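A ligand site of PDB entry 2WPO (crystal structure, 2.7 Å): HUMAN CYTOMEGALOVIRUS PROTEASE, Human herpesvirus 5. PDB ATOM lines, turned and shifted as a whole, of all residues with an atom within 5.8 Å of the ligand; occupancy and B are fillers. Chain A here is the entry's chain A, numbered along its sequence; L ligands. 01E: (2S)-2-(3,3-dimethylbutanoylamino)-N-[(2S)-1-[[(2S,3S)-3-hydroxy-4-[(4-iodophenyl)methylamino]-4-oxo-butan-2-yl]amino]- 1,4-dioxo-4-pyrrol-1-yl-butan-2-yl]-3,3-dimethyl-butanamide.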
ATOM      1  N   GLU A  31      18.604  -6.626  -6.709  1.00  0.00           N
ATOM      2  CA  GLU A  31      19.306  -6.547  -7.995  1.00  0.00           C
ATOM      3  C   GLU A  31      18.346  -6.401  -9.192  1.00  0.00           C
ATOM      4  O   GLU A  31      18.792  -6.258 -10.331  1.00  0.00           O
ATOM      5  CB  GLU A  31      20.285  -7.723  -8.194  1.00  0.00           C
ATOM      6  CG  GLU A  31      19.687  -9.136  -8.146  1.00  0.00           C
ATOM      7  CD  GLU A  31      20.576 -10.199  -8.807  1.00  0.00           C
ATOM      8  OE1 GLU A  31      21.037 -10.016  -9.955  1.00  0.00           O
ATOM      9  OE2 GLU A  31      20.799 -11.254  -8.171  1.00  0.00           O
ATOM     10  N   LEU A  32      17.039  -6.453  -8.925  1.00  0.00           N
ATOM     11  CA  LEU A  32      16.041  -6.299  -9.979  1.00  0.00           C
ATOM     12  C   LEU A  32      15.524  -4.843 -10.095  1.00  0.00           C
ATOM     13  O   LEU A  32      14.636  -4.549 -10.897  1.00  0.00           O
ATOM     14  CB  LEU A  32      14.872  -7.253  -9.762  1.00  0.00           C
ATOM     15  CG  LEU A  32      15.212  -8.725  -9.618  1.00  0.00           C
ATOM     16  CD1 LEU A  32      13.924  -9.530  -9.728  1.00  0.00           C
ATOM     17  CD2 LEU A  32      16.202  -9.133 -10.694  1.00  0.00           C
ATOM     18  N   ASN A  62      15.425 -18.294 -22.643  1.00  0.00           N
ATOM     19  CA  ASN A  62      15.952 -18.351 -21.280  1.00  0.00           C
ATOM     20  C   ASN A  62      17.447 -18.017 -21.200  1.00  0.00           C
ATOM     21  O   ASN A  62      18.249 -18.774 -20.677  1.00  0.00           O
ATOM     22  CB  ASN A  62      15.670 -19.728 -20.709  1.00  0.00           C
ATOM     23  CG  ASN A  62      16.160 -19.892 -19.303  1.00  0.00           C
ATOM     24  OD1 ASN A  62      16.279 -18.929 -18.537  1.00  0.00           O
ATOM     25  ND2 ASN A  62      16.470 -21.133 -18.941  1.00  0.00           N
ATOM     26  N   HIS A  63      17.826 -16.891 -21.821  1.00  0.00           N
ATOM     27  CA  HIS A  63      19.204 -16.401 -21.790  1.00  0.00           C
ATOM     28  C   HIS A  63      20.321 -17.241 -22.395  1.00  0.00           C
ATOM     29  O   HIS A  63      21.485 -16.819 -22.345  1.00  0.00           O
ATOM     30  CB  HIS A  63      19.567 -15.945 -20.389  1.00  0.00           C
ATOM     31  CG  HIS A  63      18.498 -15.114 -19.747  1.00  0.00           C
ATOM     32  ND1 HIS A  63      18.419 -13.749 -19.907  1.00  0.00           N
ATOM     33  CD2 HIS A  63      17.455 -15.461 -18.967  1.00  0.00           C
ATOM     34  CE1 HIS A  63      17.367 -13.290 -19.247  1.00  0.00           C
ATOM     35  NE2 HIS A  63      16.764 -14.310 -18.668  1.00  0.00           N
ATOM     36  N   LEU A 131       8.797 -12.912 -19.927  1.00  0.00           N
ATOM     37  CA  LEU A 131       9.753 -12.115 -20.663  1.00  0.00           C
ATOM     38  C   LEU A 131      10.803 -11.609 -19.660  1.00  0.00           C
ATOM     39  O   LEU A 131      10.476 -10.951 -18.674  1.00  0.00           O
ATOM     40  CB  LEU A 131       9.023 -10.968 -21.372  1.00  0.00           C
ATOM     41  CG  LEU A 131       9.043 -10.993 -22.911  1.00  0.00           C
ATOM     42  CD1 LEU A 131       8.682 -12.334 -23.473  1.00  0.00           C
ATOM     43  CD2 LEU A 131       8.117  -9.974 -23.446  1.00  0.00           C
ATOM     44  N   SER A 132      12.069 -11.946 -19.920  1.00  0.00           N
ATOM     45  CA  SER A 132      13.162 -11.580 -19.015  1.00  0.00           C
ATOM     46  C   SER A 132      14.342 -10.817 -19.634  1.00  0.00           C
ATOM     47  O   SER A 132      15.044 -11.329 -20.515  1.00  0.00           O
ATOM     48  CB  SER A 132      13.671 -12.832 -18.284  1.00  0.00           C
ATOM     49  OG  SER A 132      14.706 -12.483 -17.391  1.00  0.00           O
ATOM     50  N   LEU A 133      14.581  -9.620 -19.104  1.00  0.00           N
ATOM     51  CA  LEU A 133      15.640  -8.733 -19.561  1.00  0.00           C
ATOM     52  C   LEU A 133      16.991  -9.081 -19.002  1.00  0.00           C
ATOM     53  O   LEU A 133      17.143  -9.413 -17.821  1.00  0.00           O
ATOM     54  CB  LEU A 133      15.326  -7.288 -19.152  1.00  0.00           C
ATOM     55  CG  LEU A 133      16.348  -6.155 -19.356  1.00  0.00           C
ATOM     56  CD1 LEU A 133      16.540  -5.876 -20.840  1.00  0.00           C
ATOM     57  CD2 LEU A 133      15.920  -4.901 -18.627  1.00  0.00           C
ATOM     58  N   SER A 134      18.005  -8.903 -19.851  1.00  0.00           N
ATOM     59  CA  SER A 134      19.389  -9.118 -19.475  1.00  0.00           C
ATOM     60  C   SER A 134      19.953  -7.694 -19.542  1.00  0.00           C
ATOM     61  O   SER A 134      19.972  -7.077 -20.615  1.00  0.00           O
ATOM     62  CB  SER A 134      20.033  -9.995 -20.526  1.00  0.00           C
ATOM     63  OG  SER A 134      21.205 -10.621 -20.046  1.00  0.00           O
ATOM     64  N   SER A 135      20.364  -7.161 -18.407  1.00  0.00           N
ATOM     65  CA  SER A 135      20.890  -5.805 -18.359  1.00  0.00           C
ATOM     66  C   SER A 135      22.114  -5.626 -17.472  1.00  0.00           C
ATOM     67  O   SER A 135      22.550  -6.548 -16.768  1.00  0.00           O
ATOM     68  CB  SER A 135      19.770  -4.842 -17.919  1.00  0.00           C
ATOM     69  OG  SER A 135      19.241  -5.157 -16.629  1.00  0.00           O
ATOM     70  N   ARG A 136      22.703  -4.430 -17.509  1.00  0.00           N
ATOM     71  CA  ARG A 136      23.874  -4.126 -16.715  1.00  0.00           C
ATOM     72  C   ARG A 136      23.431  -4.150 -15.249  1.00  0.00           C
ATOM     73  O   ARG A 136      22.253  -4.086 -14.960  1.00  0.00           O
ATOM     74  CB  ARG A 136      24.400  -2.750 -17.091  1.00  0.00           C
ATOM     75  CG  ARG A 136      23.584  -1.605 -16.527  1.00  0.00           C
ATOM     76  CD  ARG A 136      24.098  -0.246 -17.013  1.00  0.00           C
ATOM     77  NE  ARG A 136      25.467   0.060 -16.632  1.00  0.00           N
ATOM     78  CZ  ARG A 136      26.440   0.336 -17.489  1.00  0.00           C
ATOM     79  NH1 ARG A 136      26.202   0.348 -18.797  1.00  0.00           N
ATOM     80  NH2 ARG A 136      27.652   0.600 -17.038  1.00  0.00           N
ATOM     81  N   ARG A 137      24.397  -4.244 -14.334  1.00  0.00           N
ATOM     82  CA  ARG A 137      24.060  -4.267 -12.907  1.00  0.00           C
ATOM     83  C   ARG A 137      23.717  -2.852 -12.467  1.00  0.00           C
ATOM     84  O   ARG A 137      24.609  -2.012 -12.297  1.00  0.00           O
ATOM     85  CB  ARG A 137      25.220  -4.820 -12.063  1.00  0.00           C
ATOM     86  CG  ARG A 137      25.523  -6.304 -12.290  1.00  0.00           C
ATOM     87  CD  ARG A 137      26.009  -6.987 -11.030  1.00  0.00           C
ATOM     88  NE  ARG A 137      25.275  -8.213 -10.767  1.00  0.00           N
ATOM     89  CZ  ARG A 137      24.261  -8.324  -9.895  1.00  0.00           C
ATOM     90  NH1 ARG A 137      23.859  -7.268  -9.184  1.00  0.00           N
ATOM     91  NH2 ARG A 137      23.629  -9.488  -9.756  1.00  0.00           N
ATOM     92  N   CYS A 138      22.431  -2.586 -12.323  1.00  0.00           N
ATOM     93  CA  CYS A 138      21.958  -1.276 -11.883  1.00  0.00           C
ATOM     94  C   CYS A 138      21.875  -1.287 -10.360  1.00  0.00           C
ATOM     95  O   CYS A 138      20.828  -1.638  -9.788  1.00  0.00           O
ATOM     96  CB  CYS A 138      20.572  -0.992 -12.489  1.00  0.00           C
ATOM     97  SG  CYS A 138      20.021   0.757 -12.473  1.00  0.00           S
ATOM     98  N   LYS A 156      21.566  -5.706 -22.607  1.00  0.00           N
ATOM     99  CA  LYS A 156      22.222  -6.805 -23.304  1.00  0.00           C
ATOM    100  C   LYS A 156      21.283  -7.541 -24.293  1.00  0.00           C
ATOM    101  O   LYS A 156      21.558  -7.598 -25.506  1.00  0.00           O
ATOM    102  CB  LYS A 156      22.836  -7.805 -22.295  1.00  0.00           C
ATOM    103  CG  LYS A 156      23.468  -9.037 -22.965  1.00  0.00           C
ATOM    104  CD  LYS A 156      23.501 -10.248 -22.047  1.00  0.00           C
ATOM    105  CE  LYS A 156      23.965 -11.500 -22.799  1.00  0.00           C
ATOM    106  NZ  LYS A 156      23.821 -12.760 -21.957  1.00  0.00           N
ATOM    107  N   HIS A 157      20.212  -8.128 -23.772  1.00  0.00           N
ATOM    108  CA  HIS A 157      19.263  -8.832 -24.619  1.00  0.00           C
ATOM    109  C   HIS A 157      17.994  -9.093 -23.826  1.00  0.00           C
ATOM    110  O   HIS A 157      17.902  -8.646 -22.681  1.00  0.00           O
ATOM    111  CB  HIS A 157      19.864 -10.141 -25.122  1.00  0.00           C
ATOM    112  CG  HIS A 157      19.762 -11.294 -24.165  1.00  0.00           C
ATOM    113  ND1 HIS A 157      20.611 -11.454 -23.078  1.00  0.00           N
ATOM    114  CD2 HIS A 157      18.935 -12.358 -24.153  1.00  0.00           C
ATOM    115  CE1 HIS A 157      20.310 -12.576 -22.446  1.00  0.00           C
ATOM    116  NE2 HIS A 157      19.295 -13.152 -23.078  1.00  0.00           N
ATOM    117  N   CYS A 161      11.210 -16.914 -21.291  1.00  0.00           N
ATOM    118  CA  CYS A 161      11.328 -17.955 -20.287  1.00  0.00           C
ATOM    119  C   CYS A 161       9.977 -18.220 -19.663  1.00  0.00           C
ATOM    120  O   CYS A 161       9.057 -17.445 -19.866  1.00  0.00           O
ATOM    121  CB  CYS A 161      12.292 -17.502 -19.235  1.00  0.00           C
ATOM    122  SG  CYS A 161      11.653 -16.099 -18.520  1.00  0.00           S
ATOM    123  N   SER A 162       9.858 -19.302 -18.903  1.00  0.00           N
ATOM    124  CA  SER A 162       8.597 -19.709 -18.255  1.00  0.00           C
ATOM    125  C   SER A 162       7.987 -18.631 -17.347  1.00  0.00           C
ATOM    126  O   SER A 162       6.787 -18.433 -17.341  1.00  0.00           O
ATOM    127  CB  SER A 162       8.808 -20.994 -17.468  1.00  0.00           C
ATOM    128  OG  SER A 162       9.804 -20.821 -16.492  1.00  0.00           O
ATOM    129  N   VAL A 163       8.830 -17.991 -16.549  1.00  0.00           N
ATOM    130  CA  VAL A 163       8.382 -16.937 -15.659  1.00  0.00           C
ATOM    131  C   VAL A 163       9.414 -15.821 -15.660  1.00  0.00           C
ATOM    132  O   VAL A 163      10.484 -15.947 -16.252  1.00  0.00           O
ATOM    133  CB  VAL A 163       8.216 -17.414 -14.194  1.00  0.00           C
ATOM    134  CG1 VAL A 163       6.767 -17.242 -13.716  1.00  0.00           C
ATOM    135  CG2 VAL A 163       8.725 -18.854 -14.028  1.00  0.00           C
ATOM    136  N   GLY A 164       9.133 -14.740 -14.973  1.00  0.00           N
ATOM    137  CA  GLY A 164      10.094 -13.671 -14.953  1.00  0.00           C
ATOM    138  C   GLY A 164      10.419 -13.403 -13.509  1.00  0.00           C
ATOM    139  O   GLY A 164       9.587 -13.623 -12.631  1.00  0.00           O
ATOM    140  N   ARG A 165      11.664 -13.000 -13.254  1.00  0.00           N
ATOM    141  CA  ARG A 165      12.076 -12.683 -11.893  1.00  0.00           C
ATOM    142  C   ARG A 165      11.350 -11.383 -11.531  1.00  0.00           C
ATOM    143  O   ARG A 165      11.008 -11.148 -10.362  1.00  0.00           O
ATOM    144  CB  ARG A 165      13.603 -12.583 -11.812  1.00  0.00           C
ATOM    145  CG  ARG A 165      14.311 -13.949 -11.983  1.00  0.00           C
ATOM    146  CD  ARG A 165      15.830 -13.868 -11.872  1.00  0.00           C
ATOM    147  NE  ARG A 165      16.258 -13.423 -10.550  1.00  0.00           N
ATOM    148  CZ  ARG A 165      17.206 -12.529 -10.315  1.00  0.00           C
ATOM    149  NH1 ARG A 165      17.881 -11.969 -11.314  1.00  0.00           N
ATOM    150  NH2 ARG A 165      17.416 -12.099  -9.065  1.00  0.00           N
ATOM    151  N   ARG A 166      11.074 -10.569 -12.543  1.00  0.00           N
ATOM    152  CA  ARG A 166      10.351  -9.317 -12.374  1.00  0.00           C
ATOM    153  C   ARG A 166       8.889  -9.611 -12.677  1.00  0.00           C
ATOM    154  O   ARG A 166       8.578 -10.347 -13.609  1.00  0.00           O
ATOM    155  CB  ARG A 166      10.905  -8.245 -13.335  1.00  0.00           C
ATOM    156  CG  ARG A 166      12.030  -7.407 -12.733  1.00  0.00           C
ATOM    157  CD  ARG A 166      12.569  -6.340 -13.664  1.00  0.00           C
ATOM    158  NE  ARG A 166      13.637  -6.879 -14.503  1.00  0.00           N
ATOM    159  CZ  ARG A 166      14.919  -6.555 -14.368  1.00  0.00           C
ATOM    160  NH1 ARG A 166      15.289  -5.673 -13.446  1.00  0.00           N
ATOM    161  NH2 ARG A 166      15.837  -7.146 -15.117  1.00  0.00           N
ATOM    162  N   THR A 169       5.596  -9.168 -16.159  1.00  0.00           N
ATOM    163  CA  THR A 169       6.350  -9.356 -17.389  1.00  0.00           C
ATOM    164  C   THR A 169       5.792 -10.508 -18.247  1.00  0.00           C
ATOM    165  O   THR A 169       6.537 -11.253 -18.895  1.00  0.00           O
ATOM    166  CB  THR A 169       7.863  -9.587 -17.086  1.00  0.00           C
ATOM    167  OG1 THR A 169       8.003 -10.727 -16.230  1.00  0.00           O
ATOM    168  CG2 THR A 169       8.460  -8.369 -16.377  1.00  0.00           C
ATOM    169  N   ILE A 231      10.620 -24.136 -10.880  1.00  0.00           N
ATOM    170  CA  ILE A 231      10.535 -22.786 -10.333  1.00  0.00           C
ATOM    171  C   ILE A 231       9.276 -22.776  -9.485  1.00  0.00           C
ATOM    172  O   ILE A 231       8.183 -23.130  -9.962  1.00  0.00           O
ATOM    173  CB  ILE A 231      10.433 -21.718 -11.419  1.00  0.00           C
ATOM    174  CG1 ILE A 231      11.657 -21.793 -12.314  1.00  0.00           C
ATOM    175  CG2 ILE A 231      10.326 -20.340 -10.781  1.00  0.00           C
ATOM    176  CD1 ILE A 231      11.374 -21.583 -13.777  1.00  0.00           C
HETATM  177  CA  01E L   1      24.809  -8.245 -15.689  1.00  0.00           C
HETATM  178  CB  01E L   1      25.091  -8.991 -17.017  1.00  0.00           C
HETATM  179  CG1 01E L   1      25.585 -10.405 -16.736  1.00  0.00           C
HETATM  180  CG2 01E L   1      23.818  -9.030 -17.863  1.00  0.00           C
HETATM  181  CG3 01E L   1      26.160  -8.260 -17.757  1.00  0.00           C
HETATM  182  C   01E L   1      23.739  -8.988 -14.908  1.00  0.00           C
HETATM  183  O   01E L   1      24.019 -10.057 -14.328  1.00  0.00           O
HETATM  184  N   01E L   1      22.528  -8.426 -14.850  1.00  0.00           N
HETATM  185  CA1 01E L   1      21.419  -9.053 -14.147  1.00  0.00           C
HETATM  186  CB1 01E L   1      20.763  -8.072 -13.134  1.00  0.00           C
HETATM  187 CG11 01E L   1      20.360  -6.799 -13.842  1.00  0.00           C
HETATM  188 CG21 01E L   1      19.555  -8.733 -12.471  1.00  0.00           C
HETATM  189 CG31 01E L   1      21.753  -7.724 -12.062  1.00  0.00           C
HETATM  190  C1  01E L   1      20.404  -9.604 -15.152  1.00  0.00           C
HETATM  191  O1  01E L   1      19.976  -8.908 -16.082  1.00  0.00           O
HETATM  192  N1  01E L   1      20.038 -10.866 -14.967  1.00  0.00           N
HETATM  193  CA2 01E L   1      19.104 -11.587 -15.824  1.00  0.00           C
HETATM  194  CB2 01E L   1      19.819 -12.811 -16.372  1.00  0.00           C
HETATM  195  CG  01E L   1      21.088 -12.461 -17.079  1.00  0.00           C
HETATM  196  OD1 01E L   1      21.443 -11.285 -17.159  1.00  0.00           O
HETATM  197  ND2 01E L   1      21.792 -13.463 -17.609  1.00  0.00           N
HETATM  198  CE1 01E L   1      21.473 -14.841 -17.385  1.00  0.00           C
HETATM  199  CH1 01E L   1      22.622 -15.556 -18.046  1.00  0.00           C
HETATM  200  CE2 01E L   1      22.920 -13.171 -18.453  1.00  0.00           C
HETATM  201  CH2 01E L   1      23.515 -14.532 -18.673  1.00  0.00           C
HETATM  202  C2  01E L   1      17.812 -12.037 -15.104  1.00  0.00           C
HETATM  203  O2  01E L   1      17.863 -12.724 -14.071  1.00  0.00           O
HETATM  204  N2  01E L   1      16.666 -11.714 -15.681  1.00  0.00           N
HETATM  205  CA3 01E L   1      15.392 -12.083 -15.076  1.00  0.00           C
HETATM  206  C3  01E L   1      14.472 -12.903 -16.041  1.00  0.00           C
HETATM  207  O3  01E L   1      13.146 -12.730 -15.683  1.00  0.00           O
HETATM  208  CB3 01E L   1      14.671 -10.844 -14.594  1.00  0.00           C
HETATM  209  C11 01E L   1      14.799 -14.405 -15.965  1.00  0.00           C
HETATM  210  O11 01E L   1      15.956 -14.802 -16.124  1.00  0.00           O
HETATM  211  N21 01E L   1      13.787 -15.228 -15.732  1.00  0.00           N
HETATM  212  C31 01E L   1      13.930 -16.686 -15.651  1.00  0.00           C
HETATM  213  C4  01E L   1      13.934 -17.151 -14.208  1.00  0.00           C
HETATM  214  C5  01E L   1      15.074 -17.053 -13.420  1.00  0.00           C
HETATM  215  C6  01E L   1      15.067 -17.512 -12.105  1.00  0.00           C
HETATM  216  C7  01E L   1      13.919 -18.076 -11.564  1.00  0.00           C
HETATM  217  I7  01E L   1      13.882 -18.742  -9.550  1.00  0.00           I
HETATM  218  C8  01E L   1      12.778 -18.175 -12.352  1.00  0.00           C
HETATM  219  C9  01E L   1      12.793 -17.719 -13.661  1.00  0.00           C
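Residues that only touch the ligand: Glu 31 (3.2 Å), Leu 32 (3.8 Å), Arg 136 (3.5 Å), Arg 137 (3.4 Å), Lys 156 (3.6 Å), Gly 164 (3.3 Å), Arg 166 (3.9 Å) and Ile 231 (3.6 Å). Of the 22 residues printed, 16 come within 4 Å of the ligand. The nearest printed residue that does not touch the ligand is Asn 62 (4.3 Å).
A ring nitrogen (ND1) of His 63 sits at hydrogen-bond distance from a ring nitrogen (NE2) of His 157 (3.3 Å). The backbone carbonyl oxygen (O) of Val 163 lies within hydrogen-bond range of the side-chain sulfur (SG) of Cys 161. The backbone carbonyl oxygen (O) of Ser 134 is in hydrogen-bond range of the backbone NH (N) of Lys 156 (2.9 Å). NH1 of Arg 166 sits at hydrogen-bond distance from O of Leu 32 (2.9 Å). The side-chain carboxylate (OE1) of Glu 31 lies within salt-bridge range of the guanidinium group (NH2) of Arg 137 (2.7 Å). The backbone carbonyl oxygen of Arg 166 is in hydrogen-bond range of the side-chain hydroxyl of Thr 169, 2.7 Å away. The backbone NH (N) of Ser 134 is in hydrogen-bond range of the backbone carbonyl oxygen (O) of His 157 (2.8 Å). The side-chain carboxylate of Glu 31 lies within salt-bridge range of the guanidinium group of Arg 165 (3.6 Å).
N of Arg 165 lies within hydrogen-bond range of O3 of the ligand, at 2.9 Å. A ring nitrogen (NE2) of His 63 sits at hydrogen-bond distance from an oxygen (O11) of the ligand (2.7 Å). OG of Ser 134 sits at hydrogen-bond distance from OD1 of the ligand. A nitrogen (N2) of the ligand lies within hydrogen-bond range of the backbone carbonyl oxygen (O) of Leu 133, 3.2 Å away. The backbone carbonyl oxygen (O) of Ser 135 sits at hydrogen-bond distance from a nitrogen (N) of the ligand, 2.7 Å away. The side-chain hydroxyl (OG) of Ser 132 is bonded to a carbon (C3) of the ligand, 1.4 Å away. NH1 of Arg 165 lies within hydrogen-bond range of O2 of the ligand. SG of Cys 161 sits at hydrogen-bond distance from N21 of the ligand (3.6 Å). N of Ser 135 is in hydrogen-bond range of O1 of the ligand. O of Val 163 lies within hydrogen-bond range of N21 of the ligand.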
